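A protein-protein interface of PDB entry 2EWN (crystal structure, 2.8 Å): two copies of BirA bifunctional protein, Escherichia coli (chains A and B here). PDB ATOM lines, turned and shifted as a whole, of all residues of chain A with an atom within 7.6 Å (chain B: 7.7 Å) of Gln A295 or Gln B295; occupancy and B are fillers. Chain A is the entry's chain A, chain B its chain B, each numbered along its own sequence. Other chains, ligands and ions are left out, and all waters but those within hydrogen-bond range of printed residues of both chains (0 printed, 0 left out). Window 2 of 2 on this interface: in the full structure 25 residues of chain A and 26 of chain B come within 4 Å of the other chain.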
ATOM      1  N   ALA A 144     -24.785   3.144  27.544  1.00  0.00           N
ATOM      2  CA  ALA A 144     -23.814   2.133  27.943  1.00  0.00           C
ATOM      3  C   ALA A 144     -24.448   0.897  28.599  1.00  0.00           C
ATOM      4  O   ALA A 144     -24.050  -0.254  28.352  1.00  0.00           O
ATOM      5  CB  ALA A 144     -22.795   2.760  28.891  1.00  0.00           C
ATOM      6  N   ALA A 145     -25.455   1.149  29.425  1.00  0.00           N
ATOM      7  CA  ALA A 145     -26.164   0.110  30.166  1.00  0.00           C
ATOM      8  C   ALA A 145     -27.169  -0.748  29.387  1.00  0.00           C
ATOM      9  O   ALA A 145     -27.730  -1.685  29.943  1.00  0.00           O
ATOM     10  CB  ALA A 145     -26.858   0.744  31.339  1.00  0.00           C
ATOM     11  N   ILE A 147     -26.729  -2.946  26.842  1.00  0.00           N
ATOM     12  CA  ILE A 147     -26.365  -4.335  26.622  1.00  0.00           C
ATOM     13  C   ILE A 147     -26.580  -5.100  27.929  1.00  0.00           C
ATOM     14  O   ILE A 147     -27.116  -6.205  27.916  1.00  0.00           O
ATOM     15  CB  ILE A 147     -24.913  -4.474  26.115  1.00  0.00           C
ATOM     16  CG1 ILE A 147     -24.853  -5.521  24.994  1.00  0.00           C
ATOM     17  CG2 ILE A 147     -23.986  -4.854  27.249  1.00  0.00           C
ATOM     18  CD1 ILE A 147     -25.398  -5.021  23.665  1.00  0.00           C
ATOM     19  N   GLY A 148     -26.192  -4.503  29.055  1.00  0.00           N
ATOM     20  CA  GLY A 148     -26.401  -5.168  30.324  1.00  0.00           C
ATOM     21  C   GLY A 148     -27.884  -5.450  30.524  1.00  0.00           C
ATOM     22  O   GLY A 148     -28.274  -6.525  30.954  1.00  0.00           O
ATOM     23  N   LEU A 151     -29.014  -8.604  28.765  1.00  0.00           N
ATOM     24  CA  LEU A 151     -28.613  -9.841  29.402  1.00  0.00           C
ATOM     25  C   LEU A 151     -29.506 -10.169  30.591  1.00  0.00           C
ATOM     26  O   LEU A 151     -29.866 -11.330  30.809  1.00  0.00           O
ATOM     27  CB  LEU A 151     -27.155  -9.745  29.825  1.00  0.00           C
ATOM     28  CG  LEU A 151     -26.206  -9.375  28.680  1.00  0.00           C
ATOM     29  CD1 LEU A 151     -24.765  -9.603  29.109  1.00  0.00           C
ATOM     30  CD2 LEU A 151     -26.540 -10.214  27.453  1.00  0.00           C
ATOM     31  N   TRP A 173     -26.663 -14.614  23.562  1.00  0.00           N
ATOM     32  CA  TRP A 173     -26.067 -13.298  23.734  1.00  0.00           C
ATOM     33  C   TRP A 173     -26.378 -12.439  22.514  1.00  0.00           C
ATOM     34  O   TRP A 173     -26.036 -12.809  21.386  1.00  0.00           O
ATOM     35  CB  TRP A 173     -24.557 -13.417  23.856  1.00  0.00           C
ATOM     36  CG  TRP A 173     -23.890 -12.074  24.027  1.00  0.00           C
ATOM     37  CD1 TRP A 173     -23.719 -11.384  25.195  1.00  0.00           C
ATOM     38  CD2 TRP A 173     -23.347 -11.243  22.989  1.00  0.00           C
ATOM     39  NE1 TRP A 173     -23.111 -10.177  24.951  1.00  0.00           N
ATOM     40  CE2 TRP A 173     -22.868 -10.063  23.607  1.00  0.00           C
ATOM     41  CE3 TRP A 173     -23.218 -11.379  21.599  1.00  0.00           C
ATOM     42  CZ2 TRP A 173     -22.271  -9.026  22.886  1.00  0.00           C
ATOM     43  CZ3 TRP A 173     -22.620 -10.342  20.879  1.00  0.00           C
ATOM     44  CH2 TRP A 173     -22.157  -9.184  21.527  1.00  0.00           C
ATOM     45  N   LEU A 258     -24.814  -5.095  36.358  1.00  0.00           N
ATOM     46  CA  LEU A 258     -24.672  -6.468  35.892  1.00  0.00           C
ATOM     47  C   LEU A 258     -24.110  -7.469  36.895  1.00  0.00           C
ATOM     48  O   LEU A 258     -24.405  -8.662  36.828  1.00  0.00           O
ATOM     49  CB  LEU A 258     -23.787  -6.465  34.653  1.00  0.00           C
ATOM     50  CG  LEU A 258     -24.284  -6.967  33.305  1.00  0.00           C
ATOM     51  CD1 LEU A 258     -23.071  -7.223  32.426  1.00  0.00           C
ATOM     52  CD2 LEU A 258     -25.035  -8.250  33.461  1.00  0.00           C
ATOM     53  N   LEU A 262     -24.090 -11.759  36.634  1.00  0.00           N
ATOM     54  CA  LEU A 262     -23.003 -12.435  35.947  1.00  0.00           C
ATOM     55  C   LEU A 262     -22.954 -13.949  35.975  1.00  0.00           C
ATOM     56  O   LEU A 262     -22.852 -14.586  34.924  1.00  0.00           O
ATOM     57  CB  LEU A 262     -21.665 -11.903  36.429  1.00  0.00           C
ATOM     58  CG  LEU A 262     -21.274 -10.559  35.829  1.00  0.00           C
ATOM     59  CD1 LEU A 262     -19.786 -10.425  35.912  1.00  0.00           C
ATOM     60  CD2 LEU A 262     -21.680 -10.485  34.367  1.00  0.00           C
ATOM     61  N   ILE A 292     -19.311 -14.317  28.790  1.00  0.00           N
ATOM     62  CA  ILE A 292     -19.272 -12.849  28.760  1.00  0.00           C
ATOM     63  C   ILE A 292     -18.291 -12.330  29.779  1.00  0.00           C
ATOM     64  O   ILE A 292     -17.892 -13.074  30.688  1.00  0.00           O
ATOM     65  CB  ILE A 292     -20.651 -12.217  29.065  1.00  0.00           C
ATOM     66  CG1 ILE A 292     -21.128 -12.646  30.456  1.00  0.00           C
ATOM     67  CG2 ILE A 292     -21.663 -12.619  28.013  1.00  0.00           C
ATOM     68  CD1 ILE A 292     -22.500 -12.092  30.827  1.00  0.00           C
ATOM     69  N   ASP A 293     -17.879 -11.071  29.626  1.00  0.00           N
ATOM     70  CA  ASP A 293     -16.957 -10.479  30.583  1.00  0.00           C
ATOM     71  C   ASP A 293     -17.813  -9.641  31.518  1.00  0.00           C
ATOM     72  O   ASP A 293     -19.005  -9.541  31.286  1.00  0.00           O
ATOM     73  CB  ASP A 293     -15.825  -9.689  29.880  1.00  0.00           C
ATOM     74  CG  ASP A 293     -16.308  -8.510  29.049  1.00  0.00           C
ATOM     75  OD1 ASP A 293     -17.524  -8.245  29.014  1.00  0.00           O
ATOM     76  OD2 ASP A 293     -15.437  -7.842  28.433  1.00  0.00           O
ATOM     77  N   LYS A 294     -17.261  -9.075  32.589  1.00  0.00           N
ATOM     78  CA  LYS A 294     -18.109  -8.310  33.515  1.00  0.00           C
ATOM     79  C   LYS A 294     -18.857  -7.152  32.886  1.00  0.00           C
ATOM     80  O   LYS A 294     -19.816  -6.653  33.470  1.00  0.00           O
ATOM     81  CB  LYS A 294     -17.331  -7.773  34.725  1.00  0.00           C
ATOM     82  CG  LYS A 294     -15.844  -8.006  34.724  1.00  0.00           C
ATOM     83  CD  LYS A 294     -15.059  -6.702  34.989  1.00  0.00           C
ATOM     84  CE  LYS A 294     -15.085  -6.259  36.455  1.00  0.00           C
ATOM     85  NZ  LYS A 294     -13.725  -5.798  36.913  1.00  0.00           N
ATOM     86  N   GLN A 295     -18.424  -6.704  31.711  1.00  0.00           N
ATOM     87  CA  GLN A 295     -19.105  -5.597  31.054  1.00  0.00           C
ATOM     88  C   GLN A 295     -20.240  -6.090  30.172  1.00  0.00           C
ATOM     89  O   GLN A 295     -20.994  -5.287  29.629  1.00  0.00           O
ATOM     90  CB  GLN A 295     -18.123  -4.763  30.228  1.00  0.00           C
ATOM     91  CG  GLN A 295     -17.217  -3.870  31.070  1.00  0.00           C
ATOM     92  CD  GLN A 295     -15.944  -4.579  31.511  1.00  0.00           C
ATOM     93  OE1 GLN A 295     -15.455  -4.373  32.627  1.00  0.00           O
ATOM     94  NE2 GLN A 295     -15.389  -5.412  30.623  1.00  0.00           N
ATOM     95  N   GLY A 296     -20.363  -7.406  30.025  1.00  0.00           N
ATOM     96  CA  GLY A 296     -21.423  -7.956  29.204  1.00  0.00           C
ATOM     97  C   GLY A 296     -21.000  -8.182  27.772  1.00  0.00           C
ATOM     98  O   GLY A 296     -21.814  -8.576  26.937  1.00  0.00           O
ATOM     99  N   ALA A 297     -19.728  -7.932  27.478  1.00  0.00           N
ATOM    100  CA  ALA A 297     -19.223  -8.124  26.124  1.00  0.00           C
ATOM    101  C   ALA A 297     -19.078  -9.618  25.914  1.00  0.00           C
ATOM    102  O   ALA A 297     -18.830 -10.369  26.856  1.00  0.00           O
ATOM    103  CB  ALA A 297     -17.868  -7.429  25.936  1.00  0.00           C
ATOM    104  N   LEU A 298     -19.286 -10.050  24.682  1.00  0.00           N
ATOM    105  CA  LEU A 298     -19.160 -11.457  24.340  1.00  0.00           C
ATOM    106  C   LEU A 298     -17.680 -11.760  24.249  1.00  0.00           C
ATOM    107  O   LEU A 298     -16.922 -10.956  23.725  1.00  0.00           O
ATOM    108  CB  LEU A 298     -19.796 -11.721  22.975  1.00  0.00           C
ATOM    109  CG  LEU A 298     -19.321 -12.995  22.266  1.00  0.00           C
ATOM    110  CD1 LEU A 298     -19.907 -14.198  22.983  1.00  0.00           C
ATOM    111  CD2 LEU A 298     -19.739 -12.978  20.794  1.00  0.00           C
ATOM    112  N   PRO A 308     -12.971  -9.568  23.488  1.00  0.00           N
ATOM    113  CA  PRO A 308     -14.306  -9.146  23.907  1.00  0.00           C
ATOM    114  C   PRO A 308     -14.947  -8.383  22.745  1.00  0.00           C
ATOM    115  O   PRO A 308     -14.292  -7.556  22.103  1.00  0.00           O
ATOM    116  CB  PRO A 308     -14.001  -8.246  25.092  1.00  0.00           C
ATOM    117  CG  PRO A 308     -12.776  -7.547  24.644  1.00  0.00           C
ATOM    118  CD  PRO A 308     -11.949  -8.679  24.070  1.00  0.00           C
ATOM    119  N   MET A 310     -18.227  -6.021  21.884  1.00  0.00           N
ATOM    120  CA  MET A 310     -19.367  -5.340  22.472  1.00  0.00           C
ATOM    121  C   MET A 310     -20.638  -5.370  21.628  1.00  0.00           C
ATOM    122  O   MET A 310     -21.733  -5.122  22.136  1.00  0.00           O
ATOM    123  CB  MET A 310     -18.958  -3.910  22.859  1.00  0.00           C
ATOM    124  CG  MET A 310     -18.565  -2.974  21.728  1.00  0.00           C
ATOM    125  SD  MET A 310     -17.792  -1.461  22.328  1.00  0.00           S
ATOM    126  CE  MET A 310     -16.282  -2.115  23.027  1.00  0.00           C
ATOM    127  N   ALA B 144     -23.527  -0.226  22.625  1.00  0.00           N
ATOM    128  CA  ALA B 144     -22.430  -0.428  23.557  1.00  0.00           C
ATOM    129  C   ALA B 144     -21.254   0.442  23.148  1.00  0.00           C
ATOM    130  O   ALA B 144     -20.449   0.881  23.979  1.00  0.00           O
ATOM    131  CB  ALA B 144     -22.027  -1.886  23.572  1.00  0.00           C
ATOM    132  N   ALA B 145     -21.180   0.723  21.857  1.00  0.00           N
ATOM    133  CA  ALA B 145     -20.098   1.528  21.314  1.00  0.00           C
ATOM    134  C   ALA B 145     -20.328   3.042  21.309  1.00  0.00           C
ATOM    135  O   ALA B 145     -19.436   3.798  20.924  1.00  0.00           O
ATOM    136  CB  ALA B 145     -19.780   1.054  19.900  1.00  0.00           C
ATOM    137  N   ILE B 147     -20.518   5.448  23.733  1.00  0.00           N
ATOM    138  CA  ILE B 147     -19.645   6.237  24.591  1.00  0.00           C
ATOM    139  C   ILE B 147     -18.250   6.378  23.971  1.00  0.00           C
ATOM    140  O   ILE B 147     -17.732   7.483  23.847  1.00  0.00           O
ATOM    141  CB  ILE B 147     -19.561   5.590  25.995  1.00  0.00           C
ATOM    142  CG1 ILE B 147     -19.703   6.657  27.086  1.00  0.00           C
ATOM    143  CG2 ILE B 147     -18.285   4.785  26.136  1.00  0.00           C
ATOM    144  CD1 ILE B 147     -21.151   6.920  27.505  1.00  0.00           C
ATOM    145  N   GLY B 148     -17.646   5.267  23.566  1.00  0.00           N
ATOM    146  CA  GLY B 148     -16.333   5.350  22.964  1.00  0.00           C
ATOM    147  C   GLY B 148     -16.401   6.275  21.775  1.00  0.00           C
ATOM    148  O   GLY B 148     -15.459   7.016  21.480  1.00  0.00           O
ATOM    149  N   LEU B 151     -16.204   9.736  22.967  1.00  0.00           N
ATOM    150  CA  LEU B 151     -14.827  10.057  23.319  1.00  0.00           C
ATOM    151  C   LEU B 151     -13.963  10.334  22.091  1.00  0.00           C
ATOM    152  O   LEU B 151     -13.147  11.252  22.117  1.00  0.00           O
ATOM    153  CB  LEU B 151     -14.207   8.935  24.139  1.00  0.00           C
ATOM    154  CG  LEU B 151     -14.967   8.605  25.415  1.00  0.00           C
ATOM    155  CD1 LEU B 151     -14.173   7.583  26.220  1.00  0.00           C
ATOM    156  CD2 LEU B 151     -15.187   9.880  26.213  1.00  0.00           C
ATOM    157  N   TRP B 173     -15.417  14.557  29.867  1.00  0.00           N
ATOM    158  CA  TRP B 173     -15.991  13.220  29.769  1.00  0.00           C
ATOM    159  C   TRP B 173     -17.505  13.293  29.943  1.00  0.00           C
ATOM    160  O   TRP B 173     -17.973  13.795  30.951  1.00  0.00           O
ATOM    161  CB  TRP B 173     -15.384  12.278  30.827  1.00  0.00           C
ATOM    162  CG  TRP B 173     -15.926  10.911  30.669  1.00  0.00           C
ATOM    163  CD1 TRP B 173     -15.523   9.979  29.760  1.00  0.00           C
ATOM    164  CD2 TRP B 173     -16.991  10.292  31.432  1.00  0.00           C
ATOM    165  NE1 TRP B 173     -16.281   8.834  29.887  1.00  0.00           N
ATOM    166  CE2 TRP B 173     -17.190   8.998  30.900  1.00  0.00           C
ATOM    167  CE3 TRP B 173     -17.804  10.709  32.503  1.00  0.00           C
ATOM    168  CZ2 TRP B 173     -18.184   8.127  31.372  1.00  0.00           C
ATOM    169  CZ3 TRP B 173     -18.769   9.837  32.963  1.00  0.00           C
ATOM    170  CH2 TRP B 173     -18.967   8.557  32.420  1.00  0.00           C
ATOM    171  N   LEU B 258     -11.634   1.834  20.801  1.00  0.00           N
ATOM    172  CA  LEU B 258     -11.009   2.943  21.512  1.00  0.00           C
ATOM    173  C   LEU B 258      -9.499   2.849  21.636  1.00  0.00           C
ATOM    174  O   LEU B 258      -8.822   3.844  21.881  1.00  0.00           O
ATOM    175  CB  LEU B 258     -11.549   3.024  22.937  1.00  0.00           C
ATOM    176  CG  LEU B 258     -12.662   3.962  23.391  1.00  0.00           C
ATOM    177  CD1 LEU B 258     -12.607   4.026  24.913  1.00  0.00           C
ATOM    178  CD2 LEU B 258     -12.479   5.359  22.815  1.00  0.00           C
ATOM    179  N   LEU B 262      -6.809   5.765  23.547  1.00  0.00           N
ATOM    180  CA  LEU B 262      -6.625   5.758  24.985  1.00  0.00           C
ATOM    181  C   LEU B 262      -5.604   6.739  25.532  1.00  0.00           C
ATOM    182  O   LEU B 262      -5.867   7.413  26.534  1.00  0.00           O
ATOM    183  CB  LEU B 262      -6.308   4.352  25.473  1.00  0.00           C
ATOM    184  CG  LEU B 262      -7.520   3.483  25.831  1.00  0.00           C
ATOM    185  CD1 LEU B 262      -7.354   3.007  27.259  1.00  0.00           C
ATOM    186  CD2 LEU B 262      -8.821   4.259  25.714  1.00  0.00           C
ATOM    187  N   ILE B 292      -9.792   7.705  32.247  1.00  0.00           N
ATOM    188  CA  ILE B 292     -10.839   6.717  31.965  1.00  0.00           C
ATOM    189  C   ILE B 292     -10.162   5.363  31.902  1.00  0.00           C
ATOM    190  O   ILE B 292      -8.940   5.259  32.038  1.00  0.00           O
ATOM    191  CB  ILE B 292     -11.522   7.016  30.608  1.00  0.00           C
ATOM    192  CG1 ILE B 292     -10.431   7.349  29.579  1.00  0.00           C
ATOM    193  CG2 ILE B 292     -12.501   8.181  30.727  1.00  0.00           C
ATOM    194  CD1 ILE B 292     -10.837   7.104  28.139  1.00  0.00           C
ATOM    195  N   ASP B 293     -10.938   4.299  31.690  1.00  0.00           N
ATOM    196  CA  ASP B 293     -10.364   2.963  31.547  1.00  0.00           C
ATOM    197  C   ASP B 293     -10.240   2.627  30.057  1.00  0.00           C
ATOM    198  O   ASP B 293     -10.201   3.526  29.213  1.00  0.00           O
ATOM    199  CB  ASP B 293     -11.209   1.901  32.270  1.00  0.00           C
ATOM    200  CG  ASP B 293     -12.640   1.837  31.774  1.00  0.00           C
ATOM    201  OD1 ASP B 293     -12.861   1.959  30.559  1.00  0.00           O
ATOM    202  OD2 ASP B 293     -13.544   1.670  32.619  1.00  0.00           O
ATOM    203  N   LYS B 294     -10.164   1.342  29.728  1.00  0.00           N
ATOM    204  CA  LYS B 294     -10.037   0.938  28.330  1.00  0.00           C
ATOM    205  C   LYS B 294     -11.387   0.822  27.604  1.00  0.00           C
ATOM    206  O   LYS B 294     -11.432   0.795  26.373  1.00  0.00           O
ATOM    207  CB  LYS B 294      -9.278  -0.393  28.208  1.00  0.00           C
ATOM    208  CG  LYS B 294      -9.530  -1.367  29.350  1.00  0.00           C
ATOM    209  CD  LYS B 294      -8.627  -2.585  29.282  1.00  0.00           C
ATOM    210  CE  LYS B 294      -8.884  -3.512  30.453  1.00  0.00           C
ATOM    211  NZ  LYS B 294      -7.974  -4.683  30.439  1.00  0.00           N
ATOM    212  N   GLN B 295     -12.483   0.761  28.362  1.00  0.00           N
ATOM    213  CA  GLN B 295     -13.818   0.682  27.767  1.00  0.00           C
ATOM    214  C   GLN B 295     -14.448   2.067  27.752  1.00  0.00           C
ATOM    215  O   GLN B 295     -15.630   2.218  27.439  1.00  0.00           O
ATOM    216  CB  GLN B 295     -14.739  -0.274  28.542  1.00  0.00           C
ATOM    217  CG  GLN B 295     -14.365  -1.737  28.489  1.00  0.00           C
ATOM    218  CD  GLN B 295     -13.656  -2.189  29.746  1.00  0.00           C
ATOM    219  OE1 GLN B 295     -12.777  -3.053  29.695  1.00  0.00           O
ATOM    220  NE2 GLN B 295     -13.873  -1.738  30.983  1.00  0.00           N
ATOM    221  N   GLY B 296     -13.683   3.071  28.124  1.00  0.00           N
ATOM    222  CA  GLY B 296     -14.147   4.449  28.083  1.00  0.00           C
ATOM    223  C   GLY B 296     -14.909   4.925  29.322  1.00  0.00           C
ATOM    224  O   GLY B 296     -15.515   5.995  29.274  1.00  0.00           O
ATOM    225  N   ALA B 297     -14.910   4.170  30.411  1.00  0.00           N
ATOM    226  CA  ALA B 297     -15.635   4.621  31.589  1.00  0.00           C
ATOM    227  C   ALA B 297     -14.784   5.578  32.433  1.00  0.00           C
ATOM    228  O   ALA B 297     -13.603   5.311  32.644  1.00  0.00           O
ATOM    229  CB  ALA B 297     -16.078   3.426  32.415  1.00  0.00           C
ATOM    230  N   LEU B 298     -15.366   6.678  32.941  1.00  0.00           N
ATOM    231  CA  LEU B 298     -14.668   7.626  33.821  1.00  0.00           C
ATOM    232  C   LEU B 298     -14.329   6.963  35.140  1.00  0.00           C
ATOM    233  O   LEU B 298     -15.170   6.308  35.766  1.00  0.00           O
ATOM    234  CB  LEU B 298     -15.516   8.898  34.059  1.00  0.00           C
ATOM    235  CG  LEU B 298     -15.464   9.458  35.490  1.00  0.00           C
ATOM    236  CD1 LEU B 298     -14.268  10.389  35.650  1.00  0.00           C
ATOM    237  CD2 LEU B 298     -16.754  10.190  35.827  1.00  0.00           C
ATOM    238  N   PRO B 308     -15.185   2.618  38.608  1.00  0.00           N
ATOM    239  CA  PRO B 308     -15.529   3.180  37.296  1.00  0.00           C
ATOM    240  C   PRO B 308     -17.042   3.320  37.069  1.00  0.00           C
ATOM    241  O   PRO B 308     -17.804   2.389  37.345  1.00  0.00           O
ATOM    242  CB  PRO B 308     -14.859   2.202  36.332  1.00  0.00           C
ATOM    243  CG  PRO B 308     -15.049   0.882  37.009  1.00  0.00           C
ATOM    244  CD  PRO B 308     -14.962   1.163  38.514  1.00  0.00           C
ATOM    245  N   MET B 310     -20.109   4.380  34.269  1.00  0.00           N
ATOM    246  CA  MET B 310     -20.347   4.438  32.824  1.00  0.00           C
ATOM    247  C   MET B 310     -21.301   5.528  32.322  1.00  0.00           C
ATOM    248  O   MET B 310     -21.464   5.695  31.105  1.00  0.00           O
ATOM    249  CB  MET B 310     -20.870   3.089  32.330  1.00  0.00           C
ATOM    250  CG  MET B 310     -22.300   2.788  32.788  1.00  0.00           C
ATOM    251  SD  MET B 310     -22.645   1.023  32.956  1.00  0.00           S
ATOM    252  CE  MET B 310     -21.457   0.567  34.222  1.00  0.00           C
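OE1 of Gln A295 sits at hydrogen-bond distance from NE2 of Gln B295, at 3.5 Å.
OD1 of Asp B293 lies within hydrogen-bond range of N of Gln B295 (2.5 Å). The backbone NH (N) of Gln A295 sits close to the side-chain carboxylate (OD1) of Asp A293 (3.2 Å).
Ala A144 touches Met B310 (CB to O, 3.9 Å). Met A310 touches Ala B144. Met A310 touches Ala B145.
Of chain B, only Gln B295 comes within 4 Å of Gln A295. Gln B295 touches just one residue of chain A: Gln A295. Printed residues of chain A within 4 Å of Met B310: Ala A144. Of the printed residues of chain A, Ala B145 touches Met A310 (3.9 Å). Of the printed residues of chain B, Ala A144 touches Met B310. Printed residues of chain B within 4 Å of Met A310: Ala B144 and Ala B145. Of the printed residues of chain A, Ala B144 touches Met A310. Asp B293 touches none of the printed residues of chain A. Ala B297 touches none of the printed residues of chain A. The nearest residue of chain B that does not touch Gln A295 is Asp B293 (6.3 Å).
Hydrophobic or aromatic side chains of chain B within 4 Å of the printed part of chain A: Ala B144 and Met B310. Hydrophobic or aromatic side chains of chain A that line the printed part of chain B: Ala A144 and Met A310. Among the printed residues, 4 pairs touch across the chains.
Ala A144 touches Met B310, and with the chains exchanged Met A310 touches Ala B144. Gln B295 touches its own counterpart, Gln A295. Met A310 touches Ala B145, but with the chains exchanged Ala A145 does not touch Met B310 (4.5 Å). Positions printed for both chains: 144, 145, 147, 148, 151, 173, 258, 262, 292, 293, 294, 295, 296, 297, 298, 308 and 310. Of the 4 pairs that touch across the chains among the printed residues, 3 have their exchanged pair printed and touching as well.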
